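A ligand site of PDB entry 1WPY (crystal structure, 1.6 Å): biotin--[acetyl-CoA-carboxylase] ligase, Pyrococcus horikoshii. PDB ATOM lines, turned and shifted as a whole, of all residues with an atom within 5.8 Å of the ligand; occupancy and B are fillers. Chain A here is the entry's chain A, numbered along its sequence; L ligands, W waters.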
ATOM      1  N   THR A  20      -5.066  23.714  -3.810  1.00  0.00           N
ATOM      2  CA  THR A  20      -6.102  22.982  -3.107  1.00  0.00           C
ATOM      3  C   THR A  20      -5.623  21.542  -2.959  1.00  0.00           C
ATOM      4  O   THR A  20      -5.485  21.025  -1.846  1.00  0.00           O
ATOM      5  CB  THR A  20      -7.429  23.008  -3.886  1.00  0.00           C
ATOM      6  OG1 THR A  20      -7.181  22.651  -5.258  1.00  0.00           O
ATOM      7  CG2 THR A  20      -8.064  24.403  -3.830  1.00  0.00           C
ATOM      8  N   SER A  21      -5.354  20.906  -4.087  1.00  0.00           N
ATOM      9  CA  SER A  21      -4.875  19.526  -4.124  1.00  0.00           C
ATOM     10  C   SER A  21      -4.172  19.279  -5.447  1.00  0.00           C
ATOM     11  O   SER A  21      -4.714  19.596  -6.507  1.00  0.00           O
ATOM     12  CB  SER A  21      -6.065  18.564  -4.000  1.00  0.00           C
ATOM     13  OG  SER A  21      -5.727  17.274  -4.490  1.00  0.00           O
ATOM     14  N   THR A  22      -2.966  18.716  -5.392  1.00  0.00           N
ATOM     15  CA  THR A  22      -2.227  18.438  -6.618  1.00  0.00           C
ATOM     16  C   THR A  22      -2.955  17.356  -7.427  1.00  0.00           C
ATOM     17  O   THR A  22      -2.983  17.405  -8.648  1.00  0.00           O
ATOM     18  CB  THR A  22      -0.758  17.989  -6.333  1.00  0.00           C
ATOM     19  OG1 THR A  22      -0.741  16.836  -5.477  1.00  0.00           O
ATOM     20  CG2 THR A  22       0.015  19.113  -5.670  1.00  0.00           C
ATOM     21  N   ASN A  23      -3.560  16.400  -6.742  1.00  0.00           N
ATOM     22  CA  ASN A  23      -4.291  15.354  -7.451  1.00  0.00           C
ATOM     23  C   ASN A  23      -5.489  15.931  -8.189  1.00  0.00           C
ATOM     24  O   ASN A  23      -5.745  15.581  -9.343  1.00  0.00           O
ATOM     25  CB  ASN A  23      -4.747  14.266  -6.466  1.00  0.00           C
ATOM     26  CG  ASN A  23      -3.913  13.007  -6.581  1.00  0.00           C
ATOM     27  OD1 ASN A  23      -2.700  13.075  -6.754  1.00  0.00           O
ATOM     28  ND2 ASN A  23      -4.558  11.839  -6.466  1.00  0.00           N
ATOM     29  N   GLU A  24      -6.239  16.826  -7.540  1.00  0.00           N
ATOM     30  CA  GLU A  24      -7.402  17.422  -8.190  1.00  0.00           C
ATOM     31  C   GLU A  24      -6.976  18.294  -9.381  1.00  0.00           C
ATOM     32  O   GLU A  24      -7.620  18.267 -10.422  1.00  0.00           O
ATOM     33  CB  GLU A  24      -8.208  18.272  -7.201  1.00  0.00           C
ATOM     34  CG  GLU A  24      -8.879  17.483  -6.078  1.00  0.00           C
ATOM     35  CD  GLU A  24      -9.829  16.411  -6.593  1.00  0.00           C
ATOM     36  OE1 GLU A  24     -10.689  16.725  -7.454  1.00  0.00           O
ATOM     37  OE2 GLU A  24      -9.742  15.264  -6.115  1.00  0.00           O
ATOM     38  N   GLN A  42      -0.868  22.115   0.612  1.00  0.00           N
ATOM     39  CA  GLN A  42      -2.187  21.881   0.053  1.00  0.00           C
ATOM     40  C   GLN A  42      -3.212  22.288   1.095  1.00  0.00           C
ATOM     41  O   GLN A  42      -3.065  21.953   2.269  1.00  0.00           O
ATOM     42  CB  GLN A  42      -2.385  20.407  -0.296  1.00  0.00           C
ATOM     43  CG  GLN A  42      -1.396  19.844  -1.293  1.00  0.00           C
ATOM     44  CD  GLN A  42      -1.710  18.413  -1.674  1.00  0.00           C
ATOM     45  OE1 GLN A  42      -1.923  18.106  -2.848  1.00  0.00           O
ATOM     46  NE2 GLN A  42      -1.736  17.535  -0.689  1.00  0.00           N
ATOM     47  N   MET A  44      -6.498  21.529   0.723  1.00  0.00           N
ATOM     48  CA  MET A  44      -7.508  20.479   0.739  1.00  0.00           C
ATOM     49  C   MET A  44      -6.926  19.141   0.292  1.00  0.00           C
ATOM     50  O   MET A  44      -7.442  18.503  -0.620  1.00  0.00           O
ATOM     51  CB  MET A  44      -8.672  20.845  -0.192  1.00  0.00           C
ATOM     52  CG  MET A  44      -9.258  22.218   0.054  1.00  0.00           C
ATOM     53  SD  MET A  44     -10.859  22.506  -1.000  1.00  0.00           S
ATOM     54  CE  MET A  44     -12.143  21.681   0.197  1.00  0.00           C
ATOM     55  N   GLY A  45      -5.835  18.731   0.943  1.00  0.00           N
ATOM     56  CA  GLY A  45      -5.198  17.473   0.593  1.00  0.00           C
ATOM     57  C   GLY A  45      -6.134  16.299   0.804  1.00  0.00           C
ATOM     58  O   GLY A  45      -6.857  16.252   1.793  1.00  0.00           O
ATOM     59  N   HIS A  46      -6.108  15.346  -0.134  1.00  0.00           N
ATOM     60  CA  HIS A  46      -6.975  14.186  -0.050  1.00  0.00           C
ATOM     61  C   HIS A  46      -6.218  12.867   0.091  1.00  0.00           C
ATOM     62  O   HIS A  46      -5.194  12.653  -0.540  1.00  0.00           O
ATOM     63  CB  HIS A  46      -7.857  14.105  -1.299  1.00  0.00           C
ATOM     64  CG  HIS A  46      -8.669  15.344  -1.537  1.00  0.00           C
ATOM     65  ND1 HIS A  46      -9.613  15.805  -0.643  1.00  0.00           N
ATOM     66  CD2 HIS A  46      -8.679  16.220  -2.572  1.00  0.00           C
ATOM     67  CE1 HIS A  46     -10.162  16.912  -1.110  1.00  0.00           C
ATOM     68  NE2 HIS A  46      -9.611  17.179  -2.280  1.00  0.00           N
ATOM     69  N   GLY A  47      -6.755  12.000   0.945  1.00  0.00           N
ATOM     70  CA  GLY A  47      -6.154  10.699   1.150  1.00  0.00           C
ATOM     71  C   GLY A  47      -7.098   9.655   0.591  1.00  0.00           C
ATOM     72  O   GLY A  47      -8.114   9.992   0.001  1.00  0.00           O
ATOM     73  N   ARG A  48      -6.762   8.383   0.787  1.00  0.00           N
ATOM     74  CA  ARG A  48      -7.603   7.297   0.300  1.00  0.00           C
ATOM     75  C   ARG A  48      -8.736   7.075   1.295  1.00  0.00           C
ATOM     76  O   ARG A  48      -8.663   7.530   2.434  1.00  0.00           O
ATOM     77  CB  ARG A  48      -6.757   6.029   0.160  1.00  0.00           C
ATOM     78  CG  ARG A  48      -7.206   5.093  -0.955  1.00  0.00           C
ATOM     79  CD  ARG A  48      -6.148   4.022  -1.196  1.00  0.00           C
ATOM     80  NE  ARG A  48      -6.048   3.088  -0.088  1.00  0.00           N
ATOM     81  CZ  ARG A  48      -6.802   1.999   0.041  1.00  0.00           C
ATOM     82  NH1 ARG A  48      -7.709   1.713  -0.886  1.00  0.00           N
ATOM     83  NH2 ARG A  48      -6.656   1.200   1.093  1.00  0.00           N
ATOM     84  N   LEU A  49      -9.785   6.375   0.859  1.00  0.00           N
ATOM     85  CA  LEU A  49     -10.919   6.108   1.733  1.00  0.00           C
ATOM     86  C   LEU A  49     -11.574   7.412   2.195  1.00  0.00           C
ATOM     87  O   LEU A  49     -12.053   7.521   3.321  1.00  0.00           O
ATOM     88  CB  LEU A  49     -10.492   5.281   2.951  1.00  0.00           C
ATOM     89  CG  LEU A  49     -10.176   3.795   2.747  1.00  0.00           C
ATOM     90  CD1 LEU A  49     -11.455   3.026   2.481  1.00  0.00           C
ATOM     91  CD2 LEU A  49      -9.189   3.617   1.600  1.00  0.00           C
ATOM     92  N   TRP A  53      -5.841  14.647   3.980  1.00  0.00           N
ATOM     93  CA  TRP A  53      -4.404  14.484   4.165  1.00  0.00           C
ATOM     94  C   TRP A  53      -3.762  15.825   4.502  1.00  0.00           C
ATOM     95  O   TRP A  53      -3.753  16.740   3.680  1.00  0.00           O
ATOM     96  CB  TRP A  53      -3.791  13.898   2.887  1.00  0.00           C
ATOM     97  CG  TRP A  53      -2.291  13.800   2.901  1.00  0.00           C
ATOM     98  CD1 TRP A  53      -1.404  14.719   2.433  1.00  0.00           C
ATOM     99  CD2 TRP A  53      -1.514  12.718   3.422  1.00  0.00           C
ATOM    100  NE1 TRP A  53      -0.118  14.283   2.635  1.00  0.00           N
ATOM    101  CE2 TRP A  53      -0.153  13.062   3.240  1.00  0.00           C
ATOM    102  CE3 TRP A  53      -1.824  11.496   4.024  1.00  0.00           C
ATOM    103  CZ2 TRP A  53       0.891  12.211   3.636  1.00  0.00           C
ATOM    104  CZ3 TRP A  53      -0.785  10.661   4.424  1.00  0.00           C
ATOM    105  CH2 TRP A  53       0.559  11.027   4.226  1.00  0.00           C
ATOM    106  N   SER A  55      -1.333  18.625   4.712  1.00  0.00           N
ATOM    107  CA  SER A  55      -0.229  18.949   3.816  1.00  0.00           C
ATOM    108  C   SER A  55       0.422  20.305   4.116  1.00  0.00           C
ATOM    109  O   SER A  55       0.377  21.222   3.294  1.00  0.00           O
ATOM    110  CB  SER A  55      -0.726  18.934   2.372  1.00  0.00           C
ATOM    111  OG  SER A  55      -1.557  17.810   2.135  1.00  0.00           O
ATOM    112  N   LEU A  60       6.595  16.893   0.964  1.00  0.00           N
ATOM    113  CA  LEU A  60       6.619  16.775  -0.494  1.00  0.00           C
ATOM    114  C   LEU A  60       5.242  16.285  -0.933  1.00  0.00           C
ATOM    115  O   LEU A  60       4.862  15.146  -0.692  1.00  0.00           O
ATOM    116  CB  LEU A  60       7.712  15.788  -0.925  1.00  0.00           C
ATOM    117  CG  LEU A  60       7.992  15.718  -2.429  1.00  0.00           C
ATOM    118  CD1 LEU A  60       8.419  17.097  -2.950  1.00  0.00           C
ATOM    119  CD2 LEU A  60       9.098  14.698  -2.691  1.00  0.00           C
ATOM    120  N   TRP A  61       4.514  17.186  -1.581  1.00  0.00           N
ATOM    121  CA  TRP A  61       3.160  16.911  -2.047  1.00  0.00           C
ATOM    122  C   TRP A  61       3.146  17.014  -3.560  1.00  0.00           C
ATOM    123  O   TRP A  61       3.268  18.116  -4.105  1.00  0.00           O
ATOM    124  CB  TRP A  61       2.194  17.933  -1.425  1.00  0.00           C
ATOM    125  CG  TRP A  61       2.530  18.344  -0.006  1.00  0.00           C
ATOM    126  CD1 TRP A  61       2.778  19.606   0.446  1.00  0.00           C
ATOM    127  CD2 TRP A  61       2.619  17.483   1.149  1.00  0.00           C
ATOM    128  NE1 TRP A  61       3.020  19.599   1.800  1.00  0.00           N
ATOM    129  CE2 TRP A  61       2.933  18.305   2.249  1.00  0.00           C
ATOM    130  CE3 TRP A  61       2.478  16.096   1.345  1.00  0.00           C
ATOM    131  CZ2 TRP A  61       3.100  17.793   3.546  1.00  0.00           C
ATOM    132  CZ3 TRP A  61       2.644  15.597   2.636  1.00  0.00           C
ATOM    133  CH2 TRP A  61       2.958  16.441   3.717  1.00  0.00           C
ATOM    134  N   LEU A  62       3.016  15.896  -4.248  1.00  0.00           N
ATOM    135  CA  LEU A  62       3.024  15.950  -5.697  1.00  0.00           C
ATOM    136  C   LEU A  62       2.136  14.920  -6.364  1.00  0.00           C
ATOM    137  O   LEU A  62       1.707  13.945  -5.734  1.00  0.00           O
ATOM    138  CB  LEU A  62       4.453  15.800  -6.214  1.00  0.00           C
ATOM    139  CG  LEU A  62       5.210  14.512  -5.842  1.00  0.00           C
ATOM    140  CD1 LEU A  62       4.815  13.357  -6.745  1.00  0.00           C
ATOM    141  CD2 LEU A  62       6.703  14.777  -5.971  1.00  0.00           C
ATOM    142  N   SER A  63       1.840  15.169  -7.627  1.00  0.00           N
ATOM    143  CA  SER A  63       1.040  14.287  -8.440  1.00  0.00           C
ATOM    144  C   SER A  63       1.701  14.201  -9.809  1.00  0.00           C
ATOM    145  O   SER A  63       2.270  15.174 -10.285  1.00  0.00           O
ATOM    146  CB  SER A  63      -0.385  14.825  -8.603  1.00  0.00           C
ATOM    147  OG  SER A  63      -1.032  14.941  -7.344  1.00  0.00           O
ATOM    148  N   ASN A 103      -0.971   1.021  -0.120  1.00  0.00           N
ATOM    149  CA  ASN A 103      -0.491   2.342  -0.572  1.00  0.00           C
ATOM    150  C   ASN A 103       0.318   3.149   0.458  1.00  0.00           C
ATOM    151  O   ASN A 103       0.648   4.312   0.233  1.00  0.00           O
ATOM    152  CB  ASN A 103      -1.709   3.166  -1.022  1.00  0.00           C
ATOM    153  CG  ASN A 103      -2.609   3.445   0.158  1.00  0.00           C
ATOM    154  OD1 ASN A 103      -2.737   2.634   1.073  1.00  0.00           O
ATOM    155  ND2 ASN A 103      -3.251   4.627   0.119  1.00  0.00           N
ATOM    156  N   ASP A 104       0.616   2.547   1.638  1.00  0.00           N
ATOM    157  CA  ASP A 104       1.341   3.351   2.646  1.00  0.00           C
ATOM    158  C   ASP A 104       2.800   2.925   2.826  1.00  0.00           C
ATOM    159  O   ASP A 104       3.168   1.792   2.566  1.00  0.00           O
ATOM    160  CB  ASP A 104       0.626   3.264   3.988  1.00  0.00           C
ATOM    161  CG  ASP A 104      -0.833   3.680   3.858  1.00  0.00           C
ATOM    162  OD1 ASP A 104      -1.081   4.737   3.286  1.00  0.00           O
ATOM    163  OD2 ASP A 104      -1.676   2.995   4.406  1.00  0.00           O
ATOM    164  N   LYS A 111       3.412   6.025   9.864  1.00  0.00           N
ATOM    165  CA  LYS A 111       3.231   6.479   8.491  1.00  0.00           C
ATOM    166  C   LYS A 111       4.071   7.695   8.096  1.00  0.00           C
ATOM    167  O   LYS A 111       3.973   8.761   8.706  1.00  0.00           O
ATOM    168  CB  LYS A 111       1.756   6.774   8.228  1.00  0.00           C
ATOM    169  CG  LYS A 111       1.424   7.047   6.779  1.00  0.00           C
ATOM    170  CD  LYS A 111      -0.078   7.107   6.570  1.00  0.00           C
ATOM    171  CE  LYS A 111      -0.439   7.276   5.103  1.00  0.00           C
ATOM    172  NZ  LYS A 111      -1.916   7.233   4.899  1.00  0.00           N
ATOM    173  N   ALA A 113       4.545   8.248   4.495  1.00  0.00           N
ATOM    174  CA  ALA A 113       4.071   8.620   3.167  1.00  0.00           C
ATOM    175  C   ALA A 113       2.852   7.820   2.742  1.00  0.00           C
ATOM    176  O   ALA A 113       2.617   6.707   3.219  1.00  0.00           O
ATOM    177  CB  ALA A 113       5.204   8.421   2.149  1.00  0.00           C
ATOM    178  N   GLY A 114       2.069   8.410   1.854  1.00  0.00           N
ATOM    179  CA  GLY A 114       0.878   7.757   1.350  1.00  0.00           C
ATOM    180  C   GLY A 114       0.784   8.004  -0.148  1.00  0.00           C
ATOM    181  O   GLY A 114       1.236   9.034  -0.639  1.00  0.00           O
ATOM    182  N   VAL A 115       0.194   7.040  -0.863  1.00  0.00           N
ATOM    183  CA  VAL A 115       0.046   7.108  -2.315  1.00  0.00           C
ATOM    184  C   VAL A 115      -1.434   7.053  -2.689  1.00  0.00           C
ATOM    185  O   VAL A 115      -2.178   6.206  -2.198  1.00  0.00           O
ATOM    186  CB  VAL A 115       0.762   5.916  -2.980  1.00  0.00           C
ATOM    187  CG1 VAL A 115       0.617   5.989  -4.491  1.00  0.00           C
ATOM    188  CG2 VAL A 115       2.232   5.906  -2.574  1.00  0.00           C
ATOM    189  N   LEU A 116      -1.859   7.953  -3.577  1.00  0.00           N
ATOM    190  CA  LEU A 116      -3.253   8.004  -4.012  1.00  0.00           C
ATOM    191  C   LEU A 116      -3.317   8.044  -5.533  1.00  0.00           C
ATOM    192  O   LEU A 116      -2.981   9.061  -6.149  1.00  0.00           O
ATOM    193  CB  LEU A 116      -3.953   9.226  -3.444  1.00  0.00           C
ATOM    194  CG  LEU A 116      -5.411   9.435  -3.875  1.00  0.00           C
ATOM    195  CD1 LEU A 116      -6.266   8.286  -3.374  1.00  0.00           C
ATOM    196  CD2 LEU A 116      -5.928  10.759  -3.314  1.00  0.00           C
ATOM    197  N   GLY A 127      -0.627  10.247  -7.128  1.00  0.00           N
ATOM    198  CA  GLY A 127      -0.351  11.226  -6.082  1.00  0.00           C
ATOM    199  C   GLY A 127       0.480  10.633  -4.964  1.00  0.00           C
ATOM    200  O   GLY A 127       0.261   9.490  -4.561  1.00  0.00           O
ATOM    201  N   ILE A 128       1.439  11.413  -4.482  1.00  0.00           N
ATOM    202  CA  ILE A 128       2.317  10.967  -3.413  1.00  0.00           C
ATOM    203  C   ILE A 128       2.497  12.087  -2.392  1.00  0.00           C
ATOM    204  O   ILE A 128       2.779  13.224  -2.755  1.00  0.00           O
ATOM    205  CB  ILE A 128       3.721  10.586  -3.955  1.00  0.00           C
ATOM    206  CG1 ILE A 128       3.590   9.479  -4.994  1.00  0.00           C
ATOM    207  CG2 ILE A 128       4.630  10.160  -2.810  1.00  0.00           C
ATOM    208  CD1 ILE A 128       4.893   9.133  -5.697  1.00  0.00           C
ATOM    209  N   GLY A 129       2.303  11.744  -1.131  1.00  0.00           N
ATOM    210  CA  GLY A 129       2.489  12.693  -0.042  1.00  0.00           C
ATOM    211  C   GLY A 129       3.552  12.088   0.845  1.00  0.00           C
ATOM    212  O   GLY A 129       3.370  10.975   1.345  1.00  0.00           O
HETATM  213  C1  LIG L   1      -3.183   7.955   1.581  1.00  0.00           C
HETATM  214  O1  LIG L   1      -4.363   7.744   1.951  1.00  0.00           O
HETATM  215  O2  LIG L   1      -2.183   7.526   2.246  1.00  0.00           O
HETATM  216  C2  LIG L   1      -2.907   8.733   0.337  1.00  0.00           C
HETATM  217  C3  LIG L   1      -2.432  10.137   0.578  1.00  0.00           C
HETATM  218  C4  LIG L   1      -1.989  10.831  -0.688  1.00  0.00           C
HETATM  219  C5  LIG L   1      -1.520  12.252  -0.444  1.00  0.00           C
HETATM  220  C6  LIG L   1      -1.069  12.990  -1.700  1.00  0.00           C
HETATM  221  S1  LIG L   1      -0.391  14.611  -1.385  1.00  0.00           S
HETATM  222  C7  LIG L   1      -0.219  14.818  -3.170  1.00  0.00           C
HETATM  223  C8  LIG L   1      -1.609  14.380  -3.680  1.00  0.00           C
HETATM  224  N1  LIG L   1      -2.613  15.451  -3.579  1.00  0.00           N
HETATM  225  C9  LIG L   1      -3.628  15.068  -2.771  1.00  0.00           C
HETATM  226  O3  LIG L   1      -4.632  15.772  -2.481  1.00  0.00           O
HETATM  227  N2  LIG L   1      -3.406  13.803  -2.280  1.00  0.00           N
HETATM  228  C10 LIG L   1      -2.167  13.247  -2.791  1.00  0.00           C
HETATM  229  O   HOH W   1      -4.558   5.061   2.888  1.00  0.00           O
HETATM  230  O   HOH W   2      -6.333   8.258   3.930  1.00  0.00           O
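N of Asn 23 lies close to OG of Ser 21.
The backbone NH of Leu 116 sits at hydrogen-bond distance from the backbone carbonyl oxygen of Gly 127, at 2.8 Å.
The side-chain hydroxyl (OG1) of Thr 22 lies within hydrogen-bond range of the side-chain hydroxyl (OG) of Ser 63.
The backbone NH (N) of Glu 24 is in hydrogen-bond range of the side-chain hydroxyl (OG) of Ser 21, at 3.1 Å.
The backbone carbonyl oxygen (O) of Leu 62 sits at hydrogen-bond distance from the backbone NH (N) of Ile 128 (2.8 Å).
O of Trp 53 is in hydrogen-bond range of OG of Ser 55 (2.9 Å).
The backbone carbonyl oxygen (O) of Leu 116 sits at hydrogen-bond distance from the side-chain amide nitrogen (ND2) of Asn 23.
OD1 of Asn 23 is in hydrogen-bond range of OG of Ser 63 (2.6 Å).
N of Asn 23 lies close to N1 of the ligand (3.4 Å).
The side-chain carboxylate of Asp 104 sits close to an oxygen (O2) of the ligand (3.2 Å).
O of Ile 128 lies close to S1 of the ligand (3.7 Å).
Gly 45 touches the ligand (CA to O3, 3.6 Å).
Gly 47 touches the ligand.
CE3 of Trp 53 touches C3 of the ligand, at 3.8 Å.
Leu 62 touches the ligand.
Ser 63 touches the ligand (OG to C8, 3.8 Å).
Asn 103 touches the ligand (ND2 to C1, 3.6 Å).
Gly 114 touches the ligand (CA to O2, 3.2 Å).
Val 115 touches the ligand.
Leu 116 touches the ligand (CB to C4, 3.7 Å).
Gly 129 touches the ligand (N to C6, 3.6 Å).
Of the 28 residues printed, 19 come within 4 Å of the ligand.
The backbone NH (N) of His 46 sits at hydrogen-bond distance from an oxygen (O3) of the ligand, at 2.8 Å.
N of Arg 48 is in hydrogen-bond range of O1 of the ligand (2.7 Å).
OG1 of Thr 22 lies within hydrogen-bond range of N1 of the ligand.
OG of Ser 21 lies within hydrogen-bond range of O3 of the ligand (2.7 Å).
The side-chain amide oxygen of Gln 42 lies within hydrogen-bond range of a nitrogen (N1) of the ligand, at 2.8 Å.
The backbone carbonyl oxygen (O) of His 46 is in hydrogen-bond range of a nitrogen (N2) of the ligand.
NZ of Lys 111 lies within salt-bridge range of O2 of the ligand (2.7 Å).
Water W2 bridges an oxygen (O1) of the ligand (2.8 Å) and the backbone carbonyl oxygen of Arg 48 (2.9 Å).
Water W1 bridges O1 of the ligand and ND2 of Asn 103.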
